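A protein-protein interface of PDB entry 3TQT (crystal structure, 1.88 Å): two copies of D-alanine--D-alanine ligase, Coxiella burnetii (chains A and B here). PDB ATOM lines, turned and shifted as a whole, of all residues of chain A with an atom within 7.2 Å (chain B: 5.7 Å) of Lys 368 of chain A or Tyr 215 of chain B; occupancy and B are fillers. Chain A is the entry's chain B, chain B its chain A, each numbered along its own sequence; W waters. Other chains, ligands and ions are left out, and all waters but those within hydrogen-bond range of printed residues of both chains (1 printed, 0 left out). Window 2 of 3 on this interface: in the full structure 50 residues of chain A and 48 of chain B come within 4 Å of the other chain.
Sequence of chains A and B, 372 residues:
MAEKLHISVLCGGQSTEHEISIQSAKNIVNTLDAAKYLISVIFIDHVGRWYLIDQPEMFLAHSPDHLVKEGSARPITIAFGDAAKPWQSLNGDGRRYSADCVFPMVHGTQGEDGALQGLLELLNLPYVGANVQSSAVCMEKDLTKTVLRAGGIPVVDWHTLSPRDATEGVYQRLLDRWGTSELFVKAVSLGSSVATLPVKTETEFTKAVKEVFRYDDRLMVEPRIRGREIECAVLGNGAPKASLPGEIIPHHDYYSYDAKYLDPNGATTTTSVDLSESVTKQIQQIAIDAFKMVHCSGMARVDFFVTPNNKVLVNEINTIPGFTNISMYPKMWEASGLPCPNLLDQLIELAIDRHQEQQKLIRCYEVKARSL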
ATOM      1  N   GLN A 358     -14.792 -11.921  18.936  1.00  0.00           N
ATOM      2  CA  GLN A 358     -15.536 -13.156  19.183  1.00  0.00           C
ATOM      3  C   GLN A 358     -15.858 -13.907  17.893  1.00  0.00           C
ATOM      4  O   GLN A 358     -15.791 -15.136  17.866  1.00  0.00           O
ATOM      5  CB  GLN A 358     -16.829 -12.881  19.960  1.00  0.00           C
ATOM      6  CG  GLN A 358     -16.602 -12.453  21.408  1.00  0.00           C
ATOM      7  CD  GLN A 358     -15.885 -13.523  22.233  1.00  0.00           C
ATOM      8  OE1 GLN A 358     -16.068 -14.723  22.012  1.00  0.00           O
ATOM      9  NE2 GLN A 358     -15.060 -13.087  23.184  1.00  0.00           N
ATOM     10  N   LYS A 360     -14.143 -13.726  15.042  1.00  0.00           N
ATOM     11  CA  LYS A 360     -12.864 -14.223  14.592  1.00  0.00           C
ATOM     12  C   LYS A 360     -12.560 -15.557  15.282  1.00  0.00           C
ATOM     13  O   LYS A 360     -12.182 -16.527  14.634  1.00  0.00           O
ATOM     14  CB  LYS A 360     -11.784 -13.186  14.905  1.00  0.00           C
ATOM     15  CG  LYS A 360     -10.514 -13.318  14.113  1.00  0.00           C
ATOM     16  CD  LYS A 360      -9.588 -12.138  14.385  1.00  0.00           C
ATOM     17  CE  LYS A 360      -8.295 -12.237  13.573  1.00  0.00           C
ATOM     18  NZ  LYS A 360      -8.535 -12.194  12.097  1.00  0.00           N
ATOM     19  N   LEU A 361     -12.748 -15.605  16.598  1.00  0.00           N
ATOM     20  CA  LEU A 361     -12.454 -16.813  17.359  1.00  0.00           C
ATOM     21  C   LEU A 361     -13.329 -17.970  16.912  1.00  0.00           C
ATOM     22  O   LEU A 361     -12.850 -19.081  16.692  1.00  0.00           O
ATOM     23  CB  LEU A 361     -12.646 -16.561  18.859  1.00  0.00           C
ATOM     24  CG  LEU A 361     -11.661 -15.562  19.460  1.00  0.00           C
ATOM     25  CD1 LEU A 361     -12.031 -15.243  20.892  1.00  0.00           C
ATOM     26  CD2 LEU A 361     -10.250 -16.129  19.386  1.00  0.00           C
ATOM     27  N   ILE A 362     -14.621 -17.721  16.777  1.00  0.00           N
ATOM     28  CA  ILE A 362     -15.519 -18.824  16.474  1.00  0.00           C
ATOM     29  C   ILE A 362     -15.324 -19.323  15.044  1.00  0.00           C
ATOM     30  O   ILE A 362     -15.407 -20.516  14.787  1.00  0.00           O
ATOM     31  CB  ILE A 362     -16.997 -18.483  16.781  1.00  0.00           C
ATOM     32  CG1 ILE A 362     -17.747 -19.746  17.224  1.00  0.00           C
ATOM     33  CG2 ILE A 362     -17.656 -17.854  15.579  1.00  0.00           C
ATOM     34  CD1 ILE A 362     -17.065 -20.524  18.346  1.00  0.00           C
ATOM     35  N   ARG A 363     -15.039 -18.409  14.120  1.00  0.00           N
ATOM     36  CA  ARG A 363     -14.726 -18.786  12.742  1.00  0.00           C
ATOM     37  C   ARG A 363     -13.441 -19.613  12.672  1.00  0.00           C
ATOM     38  O   ARG A 363     -13.358 -20.615  11.957  1.00  0.00           O
ATOM     39  CB  ARG A 363     -14.578 -17.539  11.864  1.00  0.00           C
ATOM     40  CG  ARG A 363     -15.845 -17.110  11.124  1.00  0.00           C
ATOM     41  CD  ARG A 363     -16.830 -16.371  12.023  1.00  0.00           C
ATOM     42  NE  ARG A 363     -17.617 -15.393  11.271  1.00  0.00           N
ATOM     43  CZ  ARG A 363     -18.691 -15.694  10.546  1.00  0.00           C
ATOM     44  NH1 ARG A 363     -19.113 -16.949  10.472  1.00  0.00           N
ATOM     45  NH2 ARG A 363     -19.342 -14.740   9.893  1.00  0.00           N
ATOM     46  N   CYS A 364     -12.427 -19.185  13.412  1.00  0.00           N
ATOM     47  CA  CYS A 364     -11.166 -19.901  13.403  1.00  0.00           C
ATOM     48  C   CYS A 364     -11.352 -21.301  14.004  1.00  0.00           C
ATOM     49  O   CYS A 364     -10.832 -22.292  13.493  1.00  0.00           O
ATOM     50  CB  CYS A 364     -10.112 -19.105  14.167  1.00  0.00           C
ATOM     51  SG  CYS A 364      -8.513 -19.877  14.153  1.00  0.00           S
ATOM     52  N   TYR A 365     -12.130 -21.376  15.078  1.00  0.00           N
ATOM     53  CA  TYR A 365     -12.380 -22.646  15.746  1.00  0.00           C
ATOM     54  C   TYR A 365     -13.179 -23.582  14.845  1.00  0.00           C
ATOM     55  O   TYR A 365     -12.833 -24.753  14.691  1.00  0.00           O
ATOM     56  CB  TYR A 365     -13.115 -22.395  17.065  1.00  0.00           C
ATOM     57  CG  TYR A 365     -13.555 -23.647  17.788  1.00  0.00           C
ATOM     58  CD1 TYR A 365     -12.622 -24.546  18.309  1.00  0.00           C
ATOM     59  CD2 TYR A 365     -14.905 -23.921  17.975  1.00  0.00           C
ATOM     60  CE1 TYR A 365     -13.031 -25.691  18.986  1.00  0.00           C
ATOM     61  CE2 TYR A 365     -15.319 -25.053  18.645  1.00  0.00           C
ATOM     62  CZ  TYR A 365     -14.387 -25.933  19.150  1.00  0.00           C
ATOM     63  OH  TYR A 365     -14.826 -27.053  19.822  1.00  0.00           O
ATOM     64  N   GLU A 366     -14.233 -23.051  14.234  1.00  0.00           N
ATOM     65  CA  GLU A 366     -15.063 -23.832  13.319  1.00  0.00           C
ATOM     66  C   GLU A 366     -14.246 -24.404  12.168  1.00  0.00           C
ATOM     67  O   GLU A 366     -14.467 -25.542  11.746  1.00  0.00           O
ATOM     68  CB  GLU A 366     -16.205 -22.973  12.772  1.00  0.00           C
ATOM     69  CG  GLU A 366     -17.227 -22.559  13.820  1.00  0.00           C
ATOM     70  CD  GLU A 366     -18.303 -21.651  13.256  1.00  0.00           C
ATOM     71  OE1 GLU A 366     -18.151 -21.191  12.105  1.00  0.00           O
ATOM     72  OE2 GLU A 366     -19.299 -21.394  13.964  1.00  0.00           O
ATOM     73  N   VAL A 367     -13.308 -23.616  11.653  1.00  0.00           N
ATOM     74  CA  VAL A 367     -12.433 -24.097  10.587  1.00  0.00           C
ATOM     75  C   VAL A 367     -11.581 -25.279  11.062  1.00  0.00           C
ATOM     76  O   VAL A 367     -11.473 -26.292  10.367  1.00  0.00           O
ATOM     77  CB  VAL A 367     -11.523 -22.976  10.019  1.00  0.00           C
ATOM     78  CG1 VAL A 367     -10.525 -23.550   9.044  1.00  0.00           C
ATOM     79  CG2 VAL A 367     -12.360 -21.902   9.347  1.00  0.00           C
ATOM     80  N   LYS A 368     -10.989 -25.152  12.247  1.00  0.00           N
ATOM     81  CA  LYS A 368     -10.116 -26.191  12.790  1.00  0.00           C
ATOM     82  C   LYS A 368     -10.866 -27.439  13.246  1.00  0.00           C
ATOM     83  O   LYS A 368     -10.462 -28.564  12.919  1.00  0.00           O
ATOM     84  CB  LYS A 368      -9.262 -25.636  13.930  1.00  0.00           C
ATOM     85  CG  LYS A 368      -8.148 -24.723  13.453  1.00  0.00           C
ATOM     86  CD  LYS A 368      -7.150 -25.494  12.593  1.00  0.00           C
ATOM     87  CE  LYS A 368      -5.985 -24.616  12.159  1.00  0.00           C
ATOM     88  NZ  LYS A 368      -4.983 -25.366  11.349  1.00  0.00           N
ATOM     89  N   ALA B 187      -9.127 -24.844  25.814  1.00  0.00           N
ATOM     90  CA  ALA B 187     -10.099 -23.757  25.810  1.00  0.00           C
ATOM     91  C   ALA B 187     -11.007 -23.932  27.030  1.00  0.00           C
ATOM     92  O   ALA B 187     -11.368 -25.063  27.389  1.00  0.00           O
ATOM     93  CB  ALA B 187     -10.921 -23.785  24.530  1.00  0.00           C
ATOM     94  N   LEU B 190     -14.698 -24.705  25.078  1.00  0.00           N
ATOM     95  CA  LEU B 190     -14.841 -25.469  23.841  1.00  0.00           C
ATOM     96  C   LEU B 190     -14.443 -26.923  24.065  1.00  0.00           C
ATOM     97  O   LEU B 190     -13.416 -27.200  24.691  1.00  0.00           O
ATOM     98  CB  LEU B 190     -13.988 -24.863  22.725  1.00  0.00           C
ATOM     99  CG  LEU B 190     -14.219 -23.381  22.447  1.00  0.00           C
ATOM    100  CD1 LEU B 190     -13.237 -22.885  21.385  1.00  0.00           C
ATOM    101  CD2 LEU B 190     -15.664 -23.143  22.022  1.00  0.00           C
ATOM    102  N   VAL B 194      -9.627 -30.208  19.072  1.00  0.00           N
ATOM    103  CA  VAL B 194      -8.799 -29.165  18.484  1.00  0.00           C
ATOM    104  C   VAL B 194      -8.384 -28.154  19.557  1.00  0.00           C
ATOM    105  O   VAL B 194      -7.320 -27.529  19.470  1.00  0.00           O
ATOM    106  CB  VAL B 194      -9.563 -28.437  17.352  1.00  0.00           C
ATOM    107  CG1 VAL B 194      -8.883 -27.129  16.989  1.00  0.00           C
ATOM    108  CG2 VAL B 194      -9.693 -29.340  16.130  1.00  0.00           C
ATOM    109  N   ALA B 195      -9.225 -28.012  20.577  1.00  0.00           N
ATOM    110  CA  ALA B 195      -9.024 -26.980  21.587  1.00  0.00           C
ATOM    111  C   ALA B 195      -8.482 -27.518  22.904  1.00  0.00           C
ATOM    112  O   ALA B 195      -8.556 -26.831  23.913  1.00  0.00           O
ATOM    113  CB  ALA B 195     -10.321 -26.211  21.826  1.00  0.00           C
ATOM    114  N   GLU B 211      -2.172 -21.156  20.170  1.00  0.00           N
ATOM    115  CA  GLU B 211      -3.148 -21.853  19.342  1.00  0.00           C
ATOM    116  C   GLU B 211      -4.551 -21.785  19.937  1.00  0.00           C
ATOM    117  O   GLU B 211      -5.513 -21.455  19.250  1.00  0.00           O
ATOM    118  CB  GLU B 211      -2.735 -23.310  19.159  1.00  0.00           C
ATOM    119  CG  GLU B 211      -3.845 -24.208  18.680  1.00  0.00           C
ATOM    120  CD  GLU B 211      -3.931 -24.301  17.176  1.00  0.00           C
ATOM    121  OE1 GLU B 211      -3.510 -23.344  16.485  1.00  0.00           O
ATOM    122  OE2 GLU B 211      -4.423 -25.340  16.687  1.00  0.00           O
ATOM    123  N   VAL B 212      -4.667 -22.093  21.223  1.00  0.00           N
ATOM    124  CA  VAL B 212      -5.977 -22.087  21.852  1.00  0.00           C
ATOM    125  C   VAL B 212      -6.596 -20.702  21.866  1.00  0.00           C
ATOM    126  O   VAL B 212      -7.815 -20.564  21.748  1.00  0.00           O
ATOM    127  CB  VAL B 212      -5.946 -22.643  23.277  1.00  0.00           C
ATOM    128  CG1 VAL B 212      -7.314 -22.431  23.937  1.00  0.00           C
ATOM    129  CG2 VAL B 212      -5.573 -24.125  23.247  1.00  0.00           C
ATOM    130  N   PHE B 213      -5.767 -19.669  21.995  1.00  0.00           N
ATOM    131  CA  PHE B 213      -6.292 -18.303  21.957  1.00  0.00           C
ATOM    132  C   PHE B 213      -6.776 -17.886  20.581  1.00  0.00           C
ATOM    133  O   PHE B 213      -7.330 -16.794  20.424  1.00  0.00           O
ATOM    134  CB  PHE B 213      -5.284 -17.292  22.466  1.00  0.00           C
ATOM    135  CG  PHE B 213      -5.185 -17.234  23.956  1.00  0.00           C
ATOM    136  CD1 PHE B 213      -6.319 -17.322  24.748  1.00  0.00           C
ATOM    137  CD2 PHE B 213      -3.952 -17.099  24.569  1.00  0.00           C
ATOM    138  CE1 PHE B 213      -6.216 -17.270  26.135  1.00  0.00           C
ATOM    139  CE2 PHE B 213      -3.854 -17.041  25.948  1.00  0.00           C
ATOM    140  CZ  PHE B 213      -4.982 -17.135  26.722  1.00  0.00           C
ATOM    141  N   ARG B 214      -6.565 -18.739  19.586  1.00  0.00           N
ATOM    142  CA  ARG B 214      -7.204 -18.521  18.295  1.00  0.00           C
ATOM    143  C   ARG B 214      -8.664 -18.989  18.316  1.00  0.00           C
ATOM    144  O   ARG B 214      -9.443 -18.636  17.439  1.00  0.00           O
ATOM    145  CB  ARG B 214      -6.450 -19.242  17.175  1.00  0.00           C
ATOM    146  CG  ARG B 214      -5.029 -18.727  16.938  1.00  0.00           C
ATOM    147  CD  ARG B 214      -4.257 -19.638  15.974  1.00  0.00           C
ATOM    148  NE  ARG B 214      -4.932 -19.816  14.688  1.00  0.00           N
ATOM    149  CZ  ARG B 214      -4.789 -19.001  13.643  1.00  0.00           C
ATOM    150  NH1 ARG B 214      -3.998 -17.938  13.730  1.00  0.00           N
ATOM    151  NH2 ARG B 214      -5.438 -19.241  12.508  1.00  0.00           N
ATOM    152  N   TYR B 215      -9.029 -19.779  19.324  1.00  0.00           N
ATOM    153  CA  TYR B 215     -10.360 -20.394  19.381  1.00  0.00           C
ATOM    154  C   TYR B 215     -11.252 -19.853  20.495  1.00  0.00           C
ATOM    155  O   TYR B 215     -12.471 -19.809  20.356  1.00  0.00           O
ATOM    156  CB  TYR B 215     -10.220 -21.893  19.603  1.00  0.00           C
ATOM    157  CG  TYR B 215      -9.283 -22.549  18.635  1.00  0.00           C
ATOM    158  CD1 TYR B 215      -9.183 -22.095  17.332  1.00  0.00           C
ATOM    159  CD2 TYR B 215      -8.498 -23.625  19.023  1.00  0.00           C
ATOM    160  CE1 TYR B 215      -8.324 -22.689  16.437  1.00  0.00           C
ATOM    161  CE2 TYR B 215      -7.631 -24.224  18.134  1.00  0.00           C
ATOM    162  CZ  TYR B 215      -7.553 -23.754  16.842  1.00  0.00           C
ATOM    163  OH  TYR B 215      -6.699 -24.347  15.947  1.00  0.00           O
ATOM    164  N   ASP B 216     -10.644 -19.491  21.612  1.00  0.00           N
ATOM    165  CA  ASP B 216     -11.405 -19.098  22.797  1.00  0.00           C
ATOM    166  C   ASP B 216     -10.690 -17.908  23.420  1.00  0.00           C
ATOM    167  O   ASP B 216      -9.486 -17.730  23.237  1.00  0.00           O
ATOM    168  CB  ASP B 216     -11.481 -20.272  23.784  1.00  0.00           C
ATOM    169  CG  ASP B 216     -12.676 -20.185  24.720  1.00  0.00           C
ATOM    170  OD1 ASP B 216     -13.193 -19.070  24.911  1.00  0.00           O
ATOM    171  OD2 ASP B 216     -13.095 -21.237  25.262  1.00  0.00           O
ATOM    172  N   ASP B 217     -11.409 -17.081  24.161  1.00  0.00           N
ATOM    173  CA  ASP B 217     -10.762 -15.895  24.708  1.00  0.00           C
ATOM    174  C   ASP B 217     -10.247 -16.138  26.116  1.00  0.00           C
ATOM    175  O   ASP B 217      -9.776 -15.230  26.791  1.00  0.00           O
ATOM    176  CB  ASP B 217     -11.692 -14.674  24.664  1.00  0.00           C
ATOM    177  CG  ASP B 217     -12.977 -14.879  25.444  1.00  0.00           C
ATOM    178  OD1 ASP B 217     -13.134 -15.925  26.108  1.00  0.00           O
ATOM    179  OD2 ASP B 217     -13.835 -13.974  25.406  1.00  0.00           O
HETATM  180  O   HOH W   1      -6.190 -21.688  12.948  1.00  0.00           O
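The side-chain amide nitrogen (NE2) of Gln 358 of chain A sits at hydrogen-bond distance from the side-chain carboxylate (OD2) of Asp 217 of chain B, at 2.7 Å. SG of Cys 364 of chain A is in hydrogen-bond range of NH2 of Arg 214 of chain B (3.5 Å).
N of Ala 187 of chain B is in hydrogen-bond range of O of Ala 195 of chain B, 2.8 Å away. OE2 of Glu 211 of chain B sits at hydrogen-bond distance from OH of Tyr 215 of chain B (2.6 Å).
Among the printed residues, merely in contact across the chains: Leu 361 of chain A with Phe 213 of chain B, Leu 361 of chain A with Arg 214 of chain B, Leu 361 of chain A with Tyr 215 of chain B, Leu 361 of chain A with Asp 216 of chain B, Leu 361 of chain A with Asp 217 of chain B, Cys 364 of chain A with Tyr 215 of chain B, Tyr 365 of chain A with Leu 190 of chain B, Tyr 365 of chain A with Ala 195 of chain B, Tyr 365 of chain A with Tyr 215 of chain B, Lys 368 of chain A with Val 194 of chain B and Lys 368 of chain A with Tyr 215 of chain B.
Lys 368 of chain A touches just these residues of chain B: Val 194 (3.4 Å) and Tyr 215 (2.9 Å). Of chain A, only Leu 361 (3.6 Å), Cys 364 (3.6 Å), Tyr 365 (3.6 Å) and Lys 368 (2.9 Å) come within 4 Å of Tyr 215 of chain B. Printed residues of chain B within 4 Å of Tyr 365 of chain A: Leu 190 (3.5 Å), Ala 195 (3.96 Å) and Tyr 215 (3.6 Å). Printed residues of chain A within 4 Å of Asp 217 of chain B: Gln 358 and Leu 361. Printed residues of chain A within 4 Å of Asp 216 of chain B: Leu 361. Printed residues of chain A within 4 Å of Leu 190 of chain B: Tyr 365 (3.5 Å). Ile 362 of chain A touches none of the printed residues of chain B. The nearest residue of chain B that does not touch Lys 368 of chain A is Glu 211 of chain B (4.8 Å). The nearest residue of chain A that does not touch Tyr 215 of chain B is Ile 362 of chain A (4.7 Å).
Of the 11 printed residues of chain B, 8 touch a printed residue of chain A. Hydrophobic or aromatic side chains of chain B within 4 Å of the printed part of chain A: Leu 190, Val 194, Ala 195 and Tyr 215. Hydrophobic or aromatic side chains of chain A within 4 Å of the printed part of chain B: Leu 361 and Tyr 365. Among the printed residues, 13 pairs touch across the chains.
No position is printed for both chains.
Water W1 bridges NH2 of Arg 214 of chain B (2.6 Å) and SG of Cys 364 of chain A (3.2 Å).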
